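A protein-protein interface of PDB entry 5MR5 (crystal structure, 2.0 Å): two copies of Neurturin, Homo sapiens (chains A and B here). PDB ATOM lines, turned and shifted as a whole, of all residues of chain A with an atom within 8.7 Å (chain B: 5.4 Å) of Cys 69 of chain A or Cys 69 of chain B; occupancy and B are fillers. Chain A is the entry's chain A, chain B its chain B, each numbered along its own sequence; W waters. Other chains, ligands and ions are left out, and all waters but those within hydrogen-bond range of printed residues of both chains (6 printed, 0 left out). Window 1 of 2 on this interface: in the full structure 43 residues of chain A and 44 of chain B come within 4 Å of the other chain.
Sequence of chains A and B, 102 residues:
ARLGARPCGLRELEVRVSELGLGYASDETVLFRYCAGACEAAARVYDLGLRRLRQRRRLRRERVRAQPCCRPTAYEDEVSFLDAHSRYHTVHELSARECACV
OD1 of Asp 47 of chain A is in salt-bridge range of NH1 of Arg 71 of chain B (2.8 Å). The guanidinium group (NE) of Arg 65 of chain A is in hydrogen-bond range of the side-chain sulfur (SG) of Cys 69 of chain B, 3.7 Å away. The backbone carbonyl oxygen of Arg 65 of chain A is in hydrogen-bond range of the guanidinium group of Arg 71 of chain B (2.9 Å). The side-chain sulfur (SG) of Cys 69 of chain A is in hydrogen-bond range of the guanidinium group (NE) of Arg 65 of chain B (3.7 Å). The side-chain sulfur of Cys 69 of chain A is disulfide-bonded to the side-chain sulfur of Cys 69 of chain B (2.1 Å). The guanidinium group (NH1) of Arg 71 of chain A is in hydrogen-bond range of the backbone carbonyl oxygen (O) of Arg 65 of chain B (2.9 Å). The guanidinium group (NH1) of Arg 71 of chain A is in hydrogen-bond range of the backbone carbonyl oxygen (O) of Gln 67 of chain B. NE of Arg 71 of chain A is in salt-bridge range of O of Val 102 of chain B, 3.1 Å away. The chain-end carboxylate (OXT) of Val 102 of chain A lies within salt-bridge range of the guanidinium group (NE) of Arg 71 of chain B (3.1 Å). The backbone NH of Gln 67 of chain A sits close to the guanidinium group of Arg 71 of chain B (3.4 Å).
Water W4 lies within hydrogen-bond range of the backbone carbonyl oxygen of Cys 35 of chain A, the backbone carbonyl oxygen of Cys 70 of chain A and the backbone NH of Arg 65 of chain B. Water W5 bridges O of Pro 72 of chain A (2.7 Å) and O of Val 102 of chain B (2.7 Å). Water W2 bridges the backbone NH (N) of Cys 70 of chain B and the guanidinium group (NE) of Arg 65 of chain A. Water W1 bridges O of Cys 70 of chain B (2.7 Å) and N of Arg 65 of chain A (2.9 Å). Water W3 bridges the backbone carbonyl oxygen of Arg 65 of chain B (2.8 Å) and the backbone carbonyl oxygen of Cys 35 of chain A (2.9 Å). Water W6 lies within hydrogen-bond range of NE of Arg 65 of chain B (2.8 Å) and N of Cys 70 of chain A (2.9 Å).
Of chain B, only Arg 65 and Cys 69 come within 4 Å of Cys 69 of chain A. Of chain A, only Arg 65 and Cys 69 come within 4 Å of Cys 69 of chain B. Of the printed residues of chain B, Ala 66 of chain A touches Arg 71 (3.99 Å). Of the printed residues of chain A, Pro 68 of chain B touches Arg 71. Printed residues of chain B within 4 Å of Pro 68 of chain A: Arg 71 (3.8 Å). Printed residues of chain B within 4 Å of Asp 47 of chain A: Arg 71. Ala 36 of chain A touches none of the printed residues of chain B. Arg 63 of chain A touches none of the printed residues of chain B. The nearest residue of chain A that does not touch Cys 69 of chain B is Arg 71 of chain A (4.7 Å). The nearest printed residue of chain B that does not touch Asp 47 of chain A is Cys 70 of chain B (8.0 Å).
Of the 10 printed residues of chain B, 7 touch a printed residue of chain A. Hydrophobic or aromatic side chains of chain B within 4 Å of the printed part of chain A: Val 102. Among the printed residues, Asp or Glu carboxylates within 4 Å of a Lys or Arg side-chain nitrogen of the other chain: Asp 47 of chain A with Arg 71 of chain B (2.8 Å).
Arg 65 of chain A touches its own counterpart, Arg 65 of chain B. Arg 65 of chain A touches Cys 69 of chain B, and with the chains exchanged Cys 69 of chain A touches Arg 65 of chain B. Arg 65 of chain A touches Cys 70 of chain B, and with the chains exchanged Cys 70 of chain A touches Arg 65 of chain B. Arg 65 of chain A touches Arg 71 of chain B, and with the chains exchanged Arg 71 of chain A touches Arg 65 of chain B.
Among the printed residues, pairs that only touch across the chains: Arg 65 of chain A with Arg 65 of chain B, Arg 65 of chain A with Cys 70 of chain B, Ala 66 of chain A with Arg 71 of chain B, Pro 68 of chain A with Arg 71 of chain B, Cys 70 of chain A with Arg 65 of chain B, Arg 71 of chain A with Pro 68 of chain B and Pro 72 of chain A with Val 102 of chain B.
N of Ala 36 of chain A lies close to SG of Cys 70 of chain A (3.7 Å). OD1 of Asp 47 of chain A is in hydrogen-bond range of N of Gln 67 of chain A. O of Arg 71 of chain A is in hydrogen-bond range of N of Ala 100 of chain A. The backbone NH of Cys 69 of chain B sits at hydrogen-bond distance from the chain-end carboxylate of Val 102 of chain B (2.8 Å). O of Arg 71 of chain B is in hydrogen-bond range of N of Ala 100 of chain B (3.0 Å). SG of Cys 99 of chain A forms a disulfide with SG of Cys 35 of chain A, at 2.1 Å.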
ATOM      1  N   CYS A   8      11.973 -11.101  19.109  1.00  0.00           N
ATOM      2  CA  CYS A   8      12.524 -11.594  20.349  1.00  0.00           C
ATOM      3  C   CYS A   8      13.034 -13.024  20.187  1.00  0.00           C
ATOM      4  O   CYS A   8      12.281 -13.930  19.819  1.00  0.00           O
ATOM      5  CB  CYS A   8      11.473 -11.533  21.470  1.00  0.00           C
ATOM      6  SG  CYS A   8      12.028 -12.283  23.021  1.00  0.00           S
ATOM      7  N   CYS A  35      18.688 -12.827  25.555  1.00  0.00           N
ATOM      8  CA  CYS A  35      17.396 -12.605  24.877  1.00  0.00           C
ATOM      9  C   CYS A  35      17.251 -11.170  24.448  1.00  0.00           C
ATOM     10  O   CYS A  35      17.383 -10.250  25.261  1.00  0.00           O
ATOM     11  CB  CYS A  35      16.239 -12.980  25.793  1.00  0.00           C
ATOM     12  SG  CYS A  35      16.254 -14.722  26.237  1.00  0.00           S
ATOM     13  N   ALA A  36      16.968 -10.980  23.164  1.00  0.00           N
ATOM     14  CA  ALA A  36      16.818  -9.643  22.600  1.00  0.00           C
ATOM     15  C   ALA A  36      15.835  -9.633  21.437  1.00  0.00           C
ATOM     16  O   ALA A  36      15.554 -10.664  20.827  1.00  0.00           O
ATOM     17  CB  ALA A  36      18.164  -9.102  22.137  1.00  0.00           C
ATOM     18  N   GLY A  37      15.348  -8.443  21.112  1.00  0.00           N
ATOM     19  CA  GLY A  37      14.448  -8.262  19.972  1.00  0.00           C
ATOM     20  C   GLY A  37      13.089  -7.690  20.329  1.00  0.00           C
ATOM     21  O   GLY A  37      12.814  -7.399  21.488  1.00  0.00           O
ATOM     22  N   ALA A  38      12.239  -7.553  19.312  1.00  0.00           N
ATOM     23  CA  ALA A  38      10.902  -6.967  19.455  1.00  0.00           C
ATOM     24  C   ALA A  38       9.838  -7.999  19.746  1.00  0.00           C
ATOM     25  O   ALA A  38       9.929  -9.148  19.331  1.00  0.00           O
ATOM     26  CB  ALA A  38      10.524  -6.231  18.190  1.00  0.00           C
ATOM     27  N   CYS A  39       8.816  -7.562  20.465  1.00  0.00           N
ATOM     28  CA  CYS A  39       7.643  -8.366  20.724  1.00  0.00           C
ATOM     29  C   CYS A  39       6.524  -7.785  19.857  1.00  0.00           C
ATOM     30  O   CYS A  39       5.941  -6.774  20.203  1.00  0.00           O
ATOM     31  CB  CYS A  39       7.302  -8.327  22.214  1.00  0.00           C
ATOM     32  SG  CYS A  39       8.546  -9.211  23.207  1.00  0.00           S
ATOM     33  N   ASP A  47      -3.579  -7.433  28.138  1.00  0.00           N
ATOM     34  CA  ASP A  47      -2.851  -6.205  27.892  1.00  0.00           C
ATOM     35  C   ASP A  47      -3.745  -5.117  27.297  1.00  0.00           C
ATOM     36  O   ASP A  47      -3.626  -3.942  27.642  1.00  0.00           O
ATOM     37  CB  ASP A  47      -1.630  -6.488  27.031  1.00  0.00           C
ATOM     38  CG  ASP A  47      -0.478  -7.068  27.848  1.00  0.00           C
ATOM     39  OD1 ASP A  47      -0.258  -6.587  28.978  1.00  0.00           O
ATOM     40  OD2 ASP A  47       0.214  -7.991  27.354  1.00  0.00           O
ATOM     41  N   ARG A  63       3.499   1.611  38.823  1.00  0.00           N
ATOM     42  CA  ARG A  63       4.037   1.194  37.528  1.00  0.00           C
ATOM     43  C   ARG A  63       3.377  -0.130  37.101  1.00  0.00           C
ATOM     44  O   ARG A  63       3.485  -1.140  37.805  1.00  0.00           O
ATOM     45  CB  ARG A  63       5.562   1.045  37.604  1.00  0.00           C
ATOM     46  CG  ARG A  63       6.304   1.466  36.342  1.00  0.00           C
ATOM     47  CD  ARG A  63       5.965   0.538  35.197  1.00  0.00           C
ATOM     48  NE  ARG A  63       6.890   0.589  34.060  1.00  0.00           N
ATOM     49  CZ  ARG A  63       6.507   0.537  32.785  1.00  0.00           C
ATOM     50  NH1 ARG A  63       7.413   0.546  31.821  1.00  0.00           N
ATOM     51  NH2 ARG A  63       5.211   0.485  32.463  1.00  0.00           N
ATOM     52  N   ARG A  65       2.906  -2.694  33.676  1.00  0.00           N
ATOM     53  CA  ARG A  65       3.341  -3.049  32.319  1.00  0.00           C
ATOM     54  C   ARG A  65       2.200  -3.677  31.541  1.00  0.00           C
ATOM     55  O   ARG A  65       1.686  -4.724  31.938  1.00  0.00           O
ATOM     56  CB  ARG A  65       4.505  -4.026  32.379  1.00  0.00           C
ATOM     57  CG  ARG A  65       5.773  -3.367  32.858  1.00  0.00           C
ATOM     58  CD  ARG A  65       6.956  -4.318  32.863  1.00  0.00           C
ATOM     59  NE  ARG A  65       8.170  -3.578  33.203  1.00  0.00           N
ATOM     60  CZ  ARG A  65       8.815  -2.782  32.360  1.00  0.00           C
ATOM     61  NH1 ARG A  65       8.411  -2.653  31.100  1.00  0.00           N
ATOM     62  NH2 ARG A  65       9.892  -2.130  32.768  1.00  0.00           N
ATOM     63  N   ALA A  66       1.819  -3.050  30.433  1.00  0.00           N
ATOM     64  CA  ALA A  66       0.689  -3.511  29.615  1.00  0.00           C
ATOM     65  C   ALA A  66       1.178  -3.967  28.242  1.00  0.00           C
ATOM     66  O   ALA A  66       0.487  -3.849  27.237  1.00  0.00           O
ATOM     67  CB  ALA A  66      -0.348  -2.412  29.480  1.00  0.00           C
ATOM     68  N   GLN A  67       2.366  -4.541  28.237  1.00  0.00           N
ATOM     69  CA  GLN A  67       3.067  -4.873  27.018  1.00  0.00           C
ATOM     70  C   GLN A  67       4.127  -5.891  27.418  1.00  0.00           C
ATOM     71  O   GLN A  67       4.769  -5.717  28.451  1.00  0.00           O
ATOM     72  CB  GLN A  67       3.717  -3.598  26.508  1.00  0.00           C
ATOM     73  CG  GLN A  67       4.737  -3.807  25.436  1.00  0.00           C
ATOM     74  CD  GLN A  67       5.225  -2.535  24.792  1.00  0.00           C
ATOM     75  OE1 GLN A  67       5.849  -2.594  23.744  1.00  0.00           O
ATOM     76  NE2 GLN A  67       4.944  -1.386  25.396  1.00  0.00           N
ATOM     77  N   PRO A  68       4.294  -6.967  26.633  1.00  0.00           N
ATOM     78  CA  PRO A  68       5.248  -8.004  27.024  1.00  0.00           C
ATOM     79  C   PRO A  68       6.703  -7.550  26.997  1.00  0.00           C
ATOM     80  O   PRO A  68       7.035  -6.579  26.333  1.00  0.00           O
ATOM     81  CB  PRO A  68       5.047  -9.117  25.997  1.00  0.00           C
ATOM     82  CG  PRO A  68       4.012  -8.656  25.038  1.00  0.00           C
ATOM     83  CD  PRO A  68       3.461  -7.351  25.486  1.00  0.00           C
ATOM     84  N   CYS A  69       7.553  -8.279  27.710  1.00  0.00           N
ATOM     85  CA  CYS A  69       8.992  -8.028  27.703  1.00  0.00           C
ATOM     86  C   CYS A  69       9.702  -9.246  27.120  1.00  0.00           C
ATOM     87  O   CYS A  69       9.366 -10.384  27.449  1.00  0.00           O
ATOM     88  CB  CYS A  69       9.481  -7.799  29.117  1.00  0.00           C
ATOM     89  SG  CYS A  69       8.966  -6.253  29.922  1.00  0.00           S
ATOM     90  N   CYS A  70      10.670  -9.008  26.244  1.00  0.00           N
ATOM     91  CA  CYS A  70      11.528 -10.082  25.743  1.00  0.00           C
ATOM     92  C   CYS A  70      12.546 -10.437  26.839  1.00  0.00           C
ATOM     93  O   CYS A  70      13.463  -9.671  27.128  1.00  0.00           O
ATOM     94  CB  CYS A  70      12.256  -9.631  24.477  1.00  0.00           C
ATOM     95  SG  CYS A  70      13.330 -10.900  23.757  1.00  0.00           S
ATOM     96  N   ARG A  71      12.356 -11.591  27.446  1.00  0.00           N
ATOM     97  CA  ARG A  71      13.181 -12.044  28.569  1.00  0.00           C
ATOM     98  C   ARG A  71      13.380 -13.541  28.503  1.00  0.00           C
ATOM     99  O   ARG A  71      12.654 -14.232  27.784  1.00  0.00           O
ATOM    100  CB  ARG A  71      12.504 -11.706  29.904  1.00  0.00           C
ATOM    101  CG  ARG A  71      12.456 -10.231  30.209  1.00  0.00           C
ATOM    102  CD  ARG A  71      13.820  -9.687  30.607  1.00  0.00           C
ATOM    103  NE  ARG A  71      14.246 -10.224  31.901  1.00  0.00           N
ATOM    104  CZ  ARG A  71      15.463 -10.082  32.407  1.00  0.00           C
ATOM    105  NH1 ARG A  71      16.391  -9.406  31.744  1.00  0.00           N
ATOM    106  NH2 ARG A  71      15.746 -10.606  33.584  1.00  0.00           N
ATOM    107  N   PRO A  72      14.371 -14.058  29.246  1.00  0.00           N
ATOM    108  CA  PRO A  72      14.533 -15.486  29.296  1.00  0.00           C
ATOM    109  C   PRO A  72      13.417 -16.167  30.073  1.00  0.00           C
ATOM    110  O   PRO A  72      12.953 -15.645  31.082  1.00  0.00           O
ATOM    111  CB  PRO A  72      15.868 -15.681  30.031  1.00  0.00           C
ATOM    112  CG  PRO A  72      16.548 -14.346  29.985  1.00  0.00           C
ATOM    113  CD  PRO A  72      15.440 -13.351  29.974  1.00  0.00           C
ATOM    114  N   THR A  73      13.031 -17.344  29.600  1.00  0.00           N
ATOM    115  CA  THR A  73      12.118 -18.227  30.316  1.00  0.00           C
ATOM    116  C   THR A  73      12.832 -19.453  30.850  1.00  0.00           C
ATOM    117  O   THR A  73      12.271 -20.226  31.633  1.00  0.00           O
ATOM    118  CB  THR A  73      10.999 -18.689  29.379  1.00  0.00           C
ATOM    119  OG1 THR A  73      11.587 -19.200  28.180  1.00  0.00           O
ATOM    120  CG2 THR A  73      10.137 -17.505  29.022  1.00  0.00           C
ATOM    121  N   CYS A  99      14.007 -18.002  25.229  1.00  0.00           N
ATOM    122  CA  CYS A  99      13.450 -16.645  25.270  1.00  0.00           C
ATOM    123  C   CYS A  99      11.952 -16.638  24.928  1.00  0.00           C
ATOM    124  O   CYS A  99      11.472 -17.469  24.144  1.00  0.00           O
ATOM    125  CB  CYS A  99      14.158 -15.754  24.262  1.00  0.00           C
ATOM    126  SG  CYS A  99      15.948 -15.708  24.464  1.00  0.00           S
ATOM    127  N   ALA A 100      11.228 -15.684  25.499  1.00  0.00           N
ATOM    128  CA  ALA A 100       9.854 -15.424  25.093  1.00  0.00           C
ATOM    129  C   ALA A 100       9.456 -14.007  25.453  1.00  0.00           C
ATOM    130  O   ALA A 100      10.125 -13.335  26.252  1.00  0.00           O
ATOM    131  CB  ALA A 100       8.895 -16.421  25.734  1.00  0.00           C
ATOM    132  N   CYS A 101       8.376 -13.565  24.821  1.00  0.00           N
ATOM    133  CA  CYS A 101       7.752 -12.305  25.137  1.00  0.00           C
ATOM    134  C   CYS A 101       6.788 -12.601  26.268  1.00  0.00           C
ATOM    135  O   CYS A 101       5.763 -13.223  26.064  1.00  0.00           O
ATOM    136  CB  CYS A 101       7.030 -11.725  23.916  1.00  0.00           C
ATOM    137  SG  CYS A 101       8.204 -11.143  22.688  1.00  0.00           S
ATOM    138  N   VAL A 102       7.148 -12.173  27.464  1.00  0.00           N
ATOM    139  CA  VAL A 102       6.396 -12.492  28.641  1.00  0.00           C
ATOM    140  C   VAL A 102       5.603 -11.268  29.035  1.00  0.00           C
ATOM    141  O   VAL A 102       4.394 -11.401  29.211  1.00  0.00           O
ATOM    142  CB  VAL A 102       7.335 -12.905  29.788  1.00  0.00           C
ATOM    143  CG1 VAL A 102       6.541 -13.271  31.023  1.00  0.00           C
ATOM    144  CG2 VAL A 102       8.182 -14.093  29.338  1.00  0.00           C
ATOM    145  OXT VAL A 102       6.167 -10.169  29.190  1.00  0.00           O
ATOM    146  N   CYS B  39      10.417  -4.548  41.017  1.00  0.00           N
ATOM    147  CA  CYS B  39      11.313  -5.687  41.065  1.00  0.00           C
ATOM    148  C   CYS B  39      12.629  -5.211  41.691  1.00  0.00           C
ATOM    149  O   CYS B  39      13.486  -4.625  41.031  1.00  0.00           O
ATOM    150  CB  CYS B  39      11.535  -6.210  39.658  1.00  0.00           C
ATOM    151  SG  CYS B  39      10.010  -6.865  38.933  1.00  0.00           S
ATOM    152  N   ARG B  65      16.846  -6.222  27.132  1.00  0.00           N
ATOM    153  CA  ARG B  65      16.391  -6.026  28.524  1.00  0.00           C
ATOM    154  C   ARG B  65      17.311  -6.720  29.523  1.00  0.00           C
ATOM    155  O   ARG B  65      17.445  -7.942  29.510  1.00  0.00           O
ATOM    156  CB  ARG B  65      14.971  -6.539  28.702  1.00  0.00           C
ATOM    157  CG  ARG B  65      13.948  -5.658  28.008  1.00  0.00           C
ATOM    158  CD  ARG B  65      12.500  -6.087  28.237  1.00  0.00           C
ATOM    159  NE  ARG B  65      11.594  -5.106  27.633  1.00  0.00           N
ATOM    160  CZ  ARG B  65      11.315  -3.917  28.168  1.00  0.00           C
ATOM    161  NH1 ARG B  65      11.838  -3.545  29.339  1.00  0.00           N
ATOM    162  NH2 ARG B  65      10.513  -3.081  27.532  1.00  0.00           N
ATOM    163  N   GLN B  67      17.107  -6.346  32.929  1.00  0.00           N
ATOM    164  CA  GLN B  67      16.419  -6.034  34.144  1.00  0.00           C
ATOM    165  C   GLN B  67      15.064  -6.725  34.030  1.00  0.00           C
ATOM    166  O   GLN B  67      14.476  -6.746  32.949  1.00  0.00           O
ATOM    167  CB  GLN B  67      16.261  -4.530  34.197  1.00  0.00           C
ATOM    168  CG  GLN B  67      15.301  -4.026  35.221  1.00  0.00           C
ATOM    169  CD  GLN B  67      15.347  -2.526  35.399  1.00  0.00           C
ATOM    170  OE1 GLN B  67      14.735  -2.009  36.320  1.00  0.00           O
ATOM    171  NE2 GLN B  67      16.057  -1.818  34.528  1.00  0.00           N
ATOM    172  N   PRO B  68      14.582  -7.332  35.129  1.00  0.00           N
ATOM    173  CA  PRO B  68      13.335  -8.086  35.033  1.00  0.00           C
ATOM    174  C   PRO B  68      12.119  -7.198  34.864  1.00  0.00           C
ATOM    175  O   PRO B  68      12.172  -6.003  35.191  1.00  0.00           O
ATOM    176  CB  PRO B  68      13.242  -8.856  36.355  1.00  0.00           C
ATOM    177  CG  PRO B  68      14.437  -8.486  37.162  1.00  0.00           C
ATOM    178  CD  PRO B  68      15.352  -7.630  36.344  1.00  0.00           C
ATOM    179  N   CYS B  69      11.037  -7.807  34.375  1.00  0.00           N
ATOM    180  CA  CYS B  69       9.740  -7.152  34.250  1.00  0.00           C
ATOM    181  C   CYS B  69       8.707  -7.822  35.149  1.00  0.00           C
ATOM    182  O   CYS B  69       8.608  -9.045  35.177  1.00  0.00           O
ATOM    183  CB  CYS B  69       9.261  -7.225  32.796  1.00  0.00           C
ATOM    184  SG  CYS B  69      10.197  -6.225  31.593  1.00  0.00           S
ATOM    185  N   CYS B  70       7.920  -7.016  35.859  1.00  0.00           N
ATOM    186  CA  CYS B  70       6.760  -7.505  36.600  1.00  0.00           C
ATOM    187  C   CYS B  70       5.612  -7.829  35.625  1.00  0.00           C
ATOM    188  O   CYS B  70       4.963  -6.931  35.074  1.00  0.00           O
ATOM    189  CB  CYS B  70       6.284  -6.469  37.621  1.00  0.00           C
ATOM    190  SG  CYS B  70       4.886  -7.030  38.612  1.00  0.00           S
ATOM    191  N   ARG B  71       5.390  -9.117  35.417  1.00  0.00           N
ATOM    192  CA  ARG B  71       4.438  -9.596  34.434  1.00  0.00           C
ATOM    193  C   ARG B  71       3.778 -10.846  34.947  1.00  0.00           C
ATOM    194  O   ARG B  71       4.301 -11.500  35.859  1.00  0.00           O
ATOM    195  CB  ARG B  71       5.134  -9.930  33.098  1.00  0.00           C
ATOM    196  CG  ARG B  71       5.654  -8.725  32.324  1.00  0.00           C
ATOM    197  CD  ARG B  71       4.517  -7.905  31.704  1.00  0.00           C
ATOM    198  NE  ARG B  71       3.863  -8.642  30.624  1.00  0.00           N
ATOM    199  CZ  ARG B  71       2.722  -8.295  30.040  1.00  0.00           C
ATOM    200  NH1 ARG B  71       2.065  -7.198  30.414  1.00  0.00           N
ATOM    201  NH2 ARG B  71       2.245  -9.049  29.062  1.00  0.00           N
ATOM    202  N   ALA B 100       5.247 -12.523  38.521  1.00  0.00           N
ATOM    203  CA  ALA B 100       6.639 -12.588  38.943  1.00  0.00           C
ATOM    204  C   ALA B 100       7.453 -11.530  38.211  1.00  0.00           C
ATOM    205  O   ALA B 100       6.990 -10.947  37.225  1.00  0.00           O
ATOM    206  CB  ALA B 100       7.206 -13.974  38.694  1.00  0.00           C
ATOM    207  N   CYS B 101       8.648 -11.278  38.733  1.00  0.00           N
ATOM    208  CA  CYS B 101       9.647 -10.469  38.066  1.00  0.00           C
ATOM    209  C   CYS B 101      10.418 -11.413  37.161  1.00  0.00           C
ATOM    210  O   CYS B 101      11.145 -12.281  37.632  1.00  0.00           O
ATOM    211  CB  CYS B 101      10.562  -9.809  39.100  1.00  0.00           C
ATOM    212  SG  CYS B 101       9.705  -8.521  40.049  1.00  0.00           S
ATOM    213  N   VAL B 102      10.209 -11.273  35.863  1.00  0.00           N
ATOM    214  CA  VAL B 102      10.749 -12.215  34.900  1.00  0.00           C
ATOM    215  C   VAL B 102      11.838 -11.490  34.143  1.00  0.00           C
ATOM    216  O   VAL B 102      12.972 -11.949  34.110  1.00  0.00           O
ATOM    217  CB  VAL B 102       9.668 -12.718  33.898  1.00  0.00           C
ATOM    218  CG1 VAL B 102      10.255 -13.706  32.903  1.00  0.00           C
ATOM    219  CG2 VAL B 102       8.495 -13.366  34.637  1.00  0.00           C
ATOM    220  OXT VAL B 102      11.594 -10.435  33.565  1.00  0.00           O
HETATM  221  O   HOH W   1       3.513  -4.683  35.698  1.00  0.00           O
HETATM  222  O   HOH W   2       8.004  -4.299  36.011  1.00  0.00           O
HETATM  223  O   HOH W   3      17.116 -10.365  28.165  1.00  0.00           O
HETATM  224  O   HOH W   4      15.533  -8.350  25.752  1.00  0.00           O
HETATM  225  O   HOH W   5      13.824 -14.433  33.332  1.00  0.00           O
HETATM  226  O   HOH W   6      11.328  -6.422  25.153  1.00  0.00           O
